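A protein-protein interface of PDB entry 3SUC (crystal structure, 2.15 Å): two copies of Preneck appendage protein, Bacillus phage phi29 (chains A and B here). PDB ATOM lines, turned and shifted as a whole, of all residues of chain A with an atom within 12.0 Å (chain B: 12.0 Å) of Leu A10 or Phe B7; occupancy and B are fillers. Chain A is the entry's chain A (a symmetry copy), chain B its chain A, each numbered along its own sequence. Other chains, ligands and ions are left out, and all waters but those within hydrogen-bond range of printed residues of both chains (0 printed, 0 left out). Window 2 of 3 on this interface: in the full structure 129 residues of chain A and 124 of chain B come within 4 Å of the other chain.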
ATOM      1  N   HIS A   6      37.280  -9.037 -13.000  1.00  0.00           N
ATOM      2  CA  HIS A   6      37.111 -10.116 -14.018  1.00  0.00           C
ATOM      3  C   HIS A   6      36.014 -11.114 -13.633  1.00  0.00           C
ATOM      4  O   HIS A   6      35.448 -11.789 -14.499  1.00  0.00           O
ATOM      5  CB  HIS A   6      38.436 -10.833 -14.261  1.00  0.00           C
ATOM      6  N   PHE A   7      35.721 -11.201 -12.335  1.00  0.00           N
ATOM      7  CA  PHE A   7      34.679 -12.094 -11.824  1.00  0.00           C
ATOM      8  C   PHE A   7      33.275 -11.560 -12.101  1.00  0.00           C
ATOM      9  O   PHE A   7      32.403 -12.303 -12.557  1.00  0.00           O
ATOM     10  CB  PHE A   7      34.871 -12.348 -10.324  1.00  0.00           C
ATOM     11  CG  PHE A   7      33.641 -12.879  -9.627  1.00  0.00           C
ATOM     12  CD1 PHE A   7      33.158 -14.158  -9.906  1.00  0.00           C
ATOM     13  CD2 PHE A   7      32.975 -12.103  -8.682  1.00  0.00           C
ATOM     14  CE1 PHE A   7      32.024 -14.650  -9.259  1.00  0.00           C
ATOM     15  CE2 PHE A   7      31.841 -12.587  -8.029  1.00  0.00           C
ATOM     16  CZ  PHE A   7      31.364 -13.861  -8.317  1.00  0.00           C
ATOM     17  N   ALA A   8      33.070 -10.275 -11.814  1.00  0.00           N
ATOM     18  CA  ALA A   8      31.782  -9.611 -12.021  1.00  0.00           C
ATOM     19  C   ALA A   8      31.320  -9.677 -13.475  1.00  0.00           C
ATOM     20  O   ALA A   8      30.121  -9.764 -13.743  1.00  0.00           O
ATOM     21  CB  ALA A   8      31.851  -8.165 -11.542  1.00  0.00           C
ATOM     22  N   ASP A   9      32.277  -9.650 -14.402  1.00  0.00           N
ATOM     23  CA  ASP A   9      32.008  -9.682 -15.842  1.00  0.00           C
ATOM     24  C   ASP A   9      31.341 -10.977 -16.309  1.00  0.00           C
ATOM     25  O   ASP A   9      30.596 -10.974 -17.292  1.00  0.00           O
ATOM     26  CB  ASP A   9      33.296  -9.447 -16.637  1.00  0.00           C
ATOM     27  CG  ASP A   9      33.915  -8.083 -16.368  1.00  0.00           C
ATOM     28  OD1 ASP A   9      33.735  -7.539 -15.256  1.00  0.00           O
ATOM     29  OD2 ASP A   9      34.596  -7.558 -17.274  1.00  0.00           O
ATOM     30  N   LEU A  10      31.621 -12.079 -15.615  1.00  0.00           N
ATOM     31  CA  LEU A  10      30.970 -13.356 -15.899  1.00  0.00           C
ATOM     32  C   LEU A  10      29.544 -13.370 -15.369  1.00  0.00           C
ATOM     33  O   LEU A  10      28.635 -13.856 -16.042  1.00  0.00           O
ATOM     34  CB  LEU A  10      31.761 -14.527 -15.308  1.00  0.00           C
ATOM     35  CG  LEU A  10      32.989 -15.053 -16.057  1.00  0.00           C
ATOM     36  CD1 LEU A  10      33.605 -16.194 -15.268  1.00  0.00           C
ATOM     37  CD2 LEU A  10      32.646 -15.514 -17.476  1.00  0.00           C
ATOM     38  N   VAL A  11      29.363 -12.835 -14.160  1.00  0.00           N
ATOM     39  CA  VAL A  11      28.043 -12.707 -13.535  1.00  0.00           C
ATOM     40  C   VAL A  11      27.139 -11.821 -14.395  1.00  0.00           C
ATOM     41  O   VAL A  11      25.984 -12.169 -14.652  1.00  0.00           O
ATOM     42  CB  VAL A  11      28.144 -12.135 -12.092  1.00  0.00           C
ATOM     43  CG1 VAL A  11      26.770 -12.060 -11.432  1.00  0.00           C
ATOM     44  CG2 VAL A  11      29.086 -12.976 -11.245  1.00  0.00           C
ATOM     45  N   ILE A  12      27.687 -10.690 -14.842  1.00  0.00           N
ATOM     46  CA  ILE A  12      26.992  -9.762 -15.734  1.00  0.00           C
ATOM     47  C   ILE A  12      26.544 -10.457 -17.025  1.00  0.00           C
ATOM     48  O   ILE A  12      25.381 -10.350 -17.416  1.00  0.00           O
ATOM     49  CB  ILE A  12      27.866  -8.506 -16.046  1.00  0.00           C
ATOM     50  CG1 ILE A  12      27.952  -7.597 -14.814  1.00  0.00           C
ATOM     51  CG2 ILE A  12      27.319  -7.725 -17.241  1.00  0.00           C
ATOM     52  CD1 ILE A  12      29.065  -6.561 -14.872  1.00  0.00           C
ATOM     53  N   GLN A  13      27.459 -11.189 -17.658  1.00  0.00           N
ATOM     54  CA  GLN A  13      27.179 -11.849 -18.937  1.00  0.00           C
ATOM     55  C   GLN A  13      26.274 -13.079 -18.823  1.00  0.00           C
ATOM     56  O   GLN A  13      25.848 -13.636 -19.840  1.00  0.00           O
ATOM     57  CB  GLN A  13      28.478 -12.182 -19.677  1.00  0.00           C
ATOM     58  CG  GLN A  13      29.078 -10.988 -20.413  1.00  0.00           C
ATOM     59  CD  GLN A  13      30.391 -11.311 -21.111  1.00  0.00           C
ATOM     60  OE1 GLN A  13      31.224 -12.054 -20.584  1.00  0.00           O
ATOM     61  NE2 GLN A  13      30.586 -10.741 -22.297  1.00  0.00           N
ATOM     62  N   VAL A  14      25.990 -13.497 -17.591  1.00  0.00           N
ATOM     63  CA  VAL A  14      24.957 -14.500 -17.329  1.00  0.00           C
ATOM     64  C   VAL A  14      23.590 -13.809 -17.342  1.00  0.00           C
ATOM     65  O   VAL A  14      22.648 -14.288 -17.979  1.00  0.00           O
ATOM     66  CB  VAL A  14      25.197 -15.255 -15.988  1.00  0.00           C
ATOM     67  CG1 VAL A  14      23.964 -16.056 -15.567  1.00  0.00           C
ATOM     68  CG2 VAL A  14      26.405 -16.177 -16.101  1.00  0.00           C
ATOM     69  N   ILE A  15      23.511 -12.675 -16.647  1.00  0.00           N
ATOM     70  CA  ILE A  15      22.303 -11.850 -16.586  1.00  0.00           C
ATOM     71  C   ILE A  15      21.936 -11.300 -17.969  1.00  0.00           C
ATOM     72  O   ILE A  15      20.765 -11.307 -18.354  1.00  0.00           O
ATOM     73  CB  ILE A  15      22.467 -10.690 -15.566  1.00  0.00           C
ATOM     74  CG1 ILE A  15      22.763 -11.245 -14.169  1.00  0.00           C
ATOM     75  CG2 ILE A  15      21.219  -9.806 -15.534  1.00  0.00           C
ATOM     76  CD1 ILE A  15      23.451 -10.265 -13.234  1.00  0.00           C
ATOM     77  N   ASP A  16      22.946 -10.847 -18.711  1.00  0.00           N
ATOM     78  CA  ASP A  16      22.760 -10.299 -20.058  1.00  0.00           C
ATOM     79  C   ASP A  16      22.213 -11.317 -21.062  1.00  0.00           C
ATOM     80  O   ASP A  16      21.730 -10.941 -22.133  1.00  0.00           O
ATOM     81  CB  ASP A  16      24.071  -9.697 -20.573  1.00  0.00           C
ATOM     82  CG  ASP A  16      24.477  -8.436 -19.823  1.00  0.00           C
ATOM     83  OD1 ASP A  16      23.715  -7.974 -18.945  1.00  0.00           O
ATOM     84  OD2 ASP A  16      25.566  -7.901 -20.120  1.00  0.00           O
ATOM     85  N   GLU A  17      22.296 -12.598 -20.713  1.00  0.00           N
ATOM     86  CA  GLU A  17      21.721 -13.668 -21.529  1.00  0.00           C
ATOM     87  C   GLU A  17      20.392 -14.175 -20.968  1.00  0.00           C
ATOM     88  O   GLU A  17      19.644 -14.868 -21.665  1.00  0.00           O
ATOM     89  CB  GLU A  17      22.715 -14.819 -21.701  1.00  0.00           C
ATOM     90  CG  GLU A  17      23.811 -14.529 -22.718  1.00  0.00           C
ATOM     91  CD  GLU A  17      24.624 -15.757 -23.080  1.00  0.00           C
ATOM     92  OE1 GLU A  17      24.675 -16.097 -24.282  1.00  0.00           O
ATOM     93  OE2 GLU A  17      25.206 -16.386 -22.167  1.00  0.00           O
ATOM     94  N   LEU A  18      20.106 -13.831 -19.712  1.00  0.00           N
ATOM     95  CA  LEU A  18      18.807 -14.119 -19.105  1.00  0.00           C
ATOM     96  C   LEU A  18      17.714 -13.269 -19.739  1.00  0.00           C
ATOM     97  O   LEU A  18      16.593 -13.746 -19.951  1.00  0.00           O
ATOM     98  CB  LEU A  18      18.834 -13.890 -17.590  1.00  0.00           C
ATOM     99  CG  LEU A  18      19.365 -15.006 -16.686  1.00  0.00           C
ATOM    100  CD1 LEU A  18      19.411 -14.521 -15.246  1.00  0.00           C
ATOM    101  CD2 LEU A  18      18.526 -16.278 -16.796  1.00  0.00           C
ATOM    102  N   LYS A  19      18.057 -12.014 -20.039  1.00  0.00           N
ATOM    103  CA  LYS A  19      17.172 -11.066 -20.726  1.00  0.00           C
ATOM    104  C   LYS A  19      15.820 -10.906 -20.024  1.00  0.00           C
ATOM    105  O   LYS A  19      14.768 -11.215 -20.593  1.00  0.00           O
ATOM    106  CB  LYS A  19      17.012 -11.437 -22.210  1.00  0.00           C
ATOM    107  CG  LYS A  19      18.260 -11.169 -23.034  1.00  0.00           C
ATOM    108  CD  LYS A  19      18.309 -12.009 -24.299  1.00  0.00           C
ATOM    109  CE  LYS A  19      19.628 -11.786 -25.028  1.00  0.00           C
ATOM    110  NZ  LYS A  19      19.840 -12.745 -26.146  1.00  0.00           N
ATOM    111  N   THR A  27      24.573  -3.572 -21.518  1.00  0.00           N
ATOM    112  CA  THR A  27      25.157  -4.748 -22.162  1.00  0.00           C
ATOM    113  C   THR A  27      26.018  -4.347 -23.362  1.00  0.00           C
ATOM    114  O   THR A  27      27.048  -4.968 -23.634  1.00  0.00           O
ATOM    115  CB  THR A  27      24.051  -5.733 -22.622  1.00  0.00           C
ATOM    116  OG1 THR A  27      23.213  -6.070 -21.511  1.00  0.00           O
ATOM    117  CG2 THR A  27      24.644  -7.013 -23.209  1.00  0.00           C
ATOM    118  N   HIS B   6      27.605 -25.242 -15.667  1.00  0.00           N
ATOM    119  CA  HIS B   6      27.295 -25.568 -14.243  1.00  0.00           C
ATOM    120  C   HIS B   6      27.471 -24.360 -13.316  1.00  0.00           C
ATOM    121  O   HIS B   6      26.875 -24.307 -12.235  1.00  0.00           O
ATOM    122  CB  HIS B   6      28.147 -26.743 -13.768  1.00  0.00           C
ATOM    123  N   PHE B   7      28.287 -23.397 -13.745  1.00  0.00           N
ATOM    124  CA  PHE B   7      28.532 -22.175 -12.976  1.00  0.00           C
ATOM    125  C   PHE B   7      27.355 -21.204 -13.049  1.00  0.00           C
ATOM    126  O   PHE B   7      26.926 -20.666 -12.026  1.00  0.00           O
ATOM    127  CB  PHE B   7      29.822 -21.490 -13.443  1.00  0.00           C
ATOM    128  CG  PHE B   7      29.931 -20.040 -13.036  1.00  0.00           C
ATOM    129  CD1 PHE B   7      30.082 -19.683 -11.696  1.00  0.00           C
ATOM    130  CD2 PHE B   7      29.897 -19.033 -13.998  1.00  0.00           C
ATOM    131  CE1 PHE B   7      30.188 -18.344 -11.321  1.00  0.00           C
ATOM    132  CE2 PHE B   7      30.002 -17.691 -13.632  1.00  0.00           C
ATOM    133  CZ  PHE B   7      30.148 -17.345 -12.293  1.00  0.00           C
ATOM    134  N   ALA B   8      26.850 -20.984 -14.263  1.00  0.00           N
ATOM    135  CA  ALA B   8      25.723 -20.082 -14.503  1.00  0.00           C
ATOM    136  C   ALA B   8      24.474 -20.489 -13.721  1.00  0.00           C
ATOM    137  O   ALA B   8      23.702 -19.631 -13.293  1.00  0.00           O
ATOM    138  CB  ALA B   8      25.421 -19.999 -15.994  1.00  0.00           C
ATOM    139  N   ASP B   9      24.296 -21.796 -13.532  1.00  0.00           N
ATOM    140  CA  ASP B   9      23.142 -22.359 -12.824  1.00  0.00           C
ATOM    141  C   ASP B   9      23.071 -21.952 -11.352  1.00  0.00           C
ATOM    142  O   ASP B   9      21.981 -21.871 -10.781  1.00  0.00           O
ATOM    143  CB  ASP B   9      23.132 -23.887 -12.940  1.00  0.00           C
ATOM    144  CG  ASP B   9      23.005 -24.370 -14.377  1.00  0.00           C
ATOM    145  OD1 ASP B   9      23.451 -23.655 -15.303  1.00  0.00           O
ATOM    146  OD2 ASP B   9      22.464 -25.477 -14.580  1.00  0.00           O
ATOM    147  N   LEU B  10      24.229 -21.711 -10.741  1.00  0.00           N
ATOM    148  CA  LEU B  10      24.289 -21.218  -9.367  1.00  0.00           C
ATOM    149  C   LEU B  10      23.935 -19.739  -9.303  1.00  0.00           C
ATOM    150  O   LEU B  10      23.210 -19.311  -8.403  1.00  0.00           O
ATOM    151  CB  LEU B  10      25.671 -21.453  -8.750  1.00  0.00           C
ATOM    152  CG  LEU B  10      26.019 -22.841  -8.204  1.00  0.00           C
ATOM    153  CD1 LEU B  10      27.438 -22.824  -7.666  1.00  0.00           C
ATOM    154  CD2 LEU B  10      25.044 -23.295  -7.116  1.00  0.00           C
ATOM    155  N   VAL B  11      24.453 -18.971 -10.262  1.00  0.00           N
ATOM    156  CA  VAL B  11      24.155 -17.541 -10.386  1.00  0.00           C
ATOM    157  C   VAL B  11      22.656 -17.335 -10.613  1.00  0.00           C
ATOM    158  O   VAL B  11      22.036 -16.486  -9.967  1.00  0.00           O
ATOM    159  CB  VAL B  11      24.970 -16.882 -11.535  1.00  0.00           C
ATOM    160  CG1 VAL B  11      24.694 -15.383 -11.616  1.00  0.00           C
ATOM    161  CG2 VAL B  11      26.458 -17.130 -11.350  1.00  0.00           C
ATOM    162  N   ILE B  12      22.090 -18.131 -11.521  1.00  0.00           N
ATOM    163  CA  ILE B  12      20.656 -18.121 -11.811  1.00  0.00           C
ATOM    164  C   ILE B  12      19.828 -18.397 -10.552  1.00  0.00           C
ATOM    165  O   ILE B  12      18.894 -17.653 -10.246  1.00  0.00           O
ATOM    166  CB  ILE B  12      20.297 -19.124 -12.952  1.00  0.00           C
ATOM    167  CG1 ILE B  12      20.795 -18.597 -14.304  1.00  0.00           C
ATOM    168  CG2 ILE B  12      18.792 -19.391 -13.012  1.00  0.00           C
ATOM    169  CD1 ILE B  12      20.844 -19.642 -15.408  1.00  0.00           C
ATOM    170  N   GLN B  13      20.193 -19.444  -9.814  1.00  0.00           N
ATOM    171  CA  GLN B  13      19.444 -19.857  -8.623  1.00  0.00           C
ATOM    172  C   GLN B  13      19.634 -18.938  -7.413  1.00  0.00           C
ATOM    173  O   GLN B  13      18.948 -19.094  -6.397  1.00  0.00           O
ATOM    174  CB  GLN B  13      19.746 -21.315  -8.266  1.00  0.00           C
ATOM    175  CG  GLN B  13      18.970 -22.319  -9.113  1.00  0.00           C
ATOM    176  CD  GLN B  13      19.304 -23.766  -8.786  1.00  0.00           C
ATOM    177  OE1 GLN B  13      20.461 -24.109  -8.526  1.00  0.00           O
ATOM    178  NE2 GLN B  13      18.290 -24.627  -8.810  1.00  0.00           N
ATOM    179  N   VAL B  14      20.563 -17.990  -7.525  1.00  0.00           N
ATOM    180  CA  VAL B  14      20.686 -16.903  -6.552  1.00  0.00           C
ATOM    181  C   VAL B  14      19.643 -15.831  -6.885  1.00  0.00           C
ATOM    182  O   VAL B  14      18.924 -15.357  -6.002  1.00  0.00           O
ATOM    183  CB  VAL B  14      22.123 -16.304  -6.520  1.00  0.00           C
ATOM    184  CG1 VAL B  14      22.161 -14.980  -5.755  1.00  0.00           C
ATOM    185  CG2 VAL B  14      23.102 -17.293  -5.899  1.00  0.00           C
ATOM    186  N   ILE B  15      19.567 -15.480  -8.168  1.00  0.00           N
ATOM    187  CA  ILE B  15      18.595 -14.511  -8.681  1.00  0.00           C
ATOM    188  C   ILE B  15      17.159 -15.010  -8.491  1.00  0.00           C
ATOM    189  O   ILE B  15      16.280 -14.246  -8.086  1.00  0.00           O
ATOM    190  CB  ILE B  15      18.865 -14.186 -10.176  1.00  0.00           C
ATOM    191  CG1 ILE B  15      20.278 -13.619 -10.353  1.00  0.00           C
ATOM    192  CG2 ILE B  15      17.826 -13.204 -10.720  1.00  0.00           C
ATOM    193  CD1 ILE B  15      20.842 -13.761 -11.756  1.00  0.00           C
ATOM    194  N   ASP B  16      16.940 -16.296  -8.766  1.00  0.00           N
ATOM    195  CA  ASP B  16      15.624 -16.925  -8.626  1.00  0.00           C
ATOM    196  C   ASP B  16      15.100 -16.936  -7.188  1.00  0.00           C
ATOM    197  O   ASP B  16      13.908 -17.153  -6.958  1.00  0.00           O
ATOM    198  CB  ASP B  16      15.653 -18.350  -9.190  1.00  0.00           C
ATOM    199  CG  ASP B  16      15.807 -18.383 -10.705  1.00  0.00           C
ATOM    200  OD1 ASP B  16      15.822 -17.307 -11.342  1.00  0.00           O
ATOM    201  OD2 ASP B  16      15.909 -19.496 -11.261  1.00  0.00           O
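No residue of chain B comes within 4 Å of His A6.
Phe A7 touches none of the printed residues of chain B.
No residue of chain B comes within 4 Å of Ala A8.
No residue of chain B comes within 4 Å of Asp A9.
Of the printed residues of chain B, Leu A10 touches Phe B7.
Val A11 touches one residue of chain B.
No residue of chain B comes within 4 Å of Ile A12.
Of the printed residues of chain B, Val A14 touches Ala B8.
Printed residues of chain B within 4 Å of Leu A18: Ile B15 (3.8 Å).
No residue of chain A comes within 4 Å of His B6.
Printed residues of chain A within 4 Å of Phe B7: Leu A10.
Ala B8 touches just one residue of chain A: Val A14 (3.9 Å).
No residue of chain A comes within 4 Å of Asp B9.
Val B11 touches one residue of chain A.
Printed residues of chain A within 4 Å of Ile B15: Ile A15 (3.98 Å) and Leu A18 (3.8 Å).
The nearest printed residue of chain A that does not touch Phe B7 is Phe A7 (4.5 Å).
Among the printed residues, merely in contact across the chains: Leu A10 with Phe B7 (3.99 Å), Val A11 with Val B11 (3.9 Å), Val A14 with Ala B8 (3.9 Å), Ile A15 with Ile B15 (3.98 Å) and Leu A18 with Ile B15 (3.8 Å).
Leu A10 touches Phe B7, but with the chains exchanged Phe A7 does not touch Leu B10 (9.3 Å).
Val B11 touches its own counterpart, Val A11.
Val A14 touches Ala B8, but with the chains exchanged Ala A8 does not touch Val B14 (12.4 Å).
Ile B15 touches its own counterpart, Ile A15.
Positions printed for both chains: 6, 7, 8, 9, 10, 11, 12, 13, 14, 15 and 16.
Hydrophobic or aromatic side chains of chain B that line the printed part of chain A: Phe B7, Ala B8, Val B11 and Ile B15.
Among the printed residues, 5 pairs touch across the chains.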
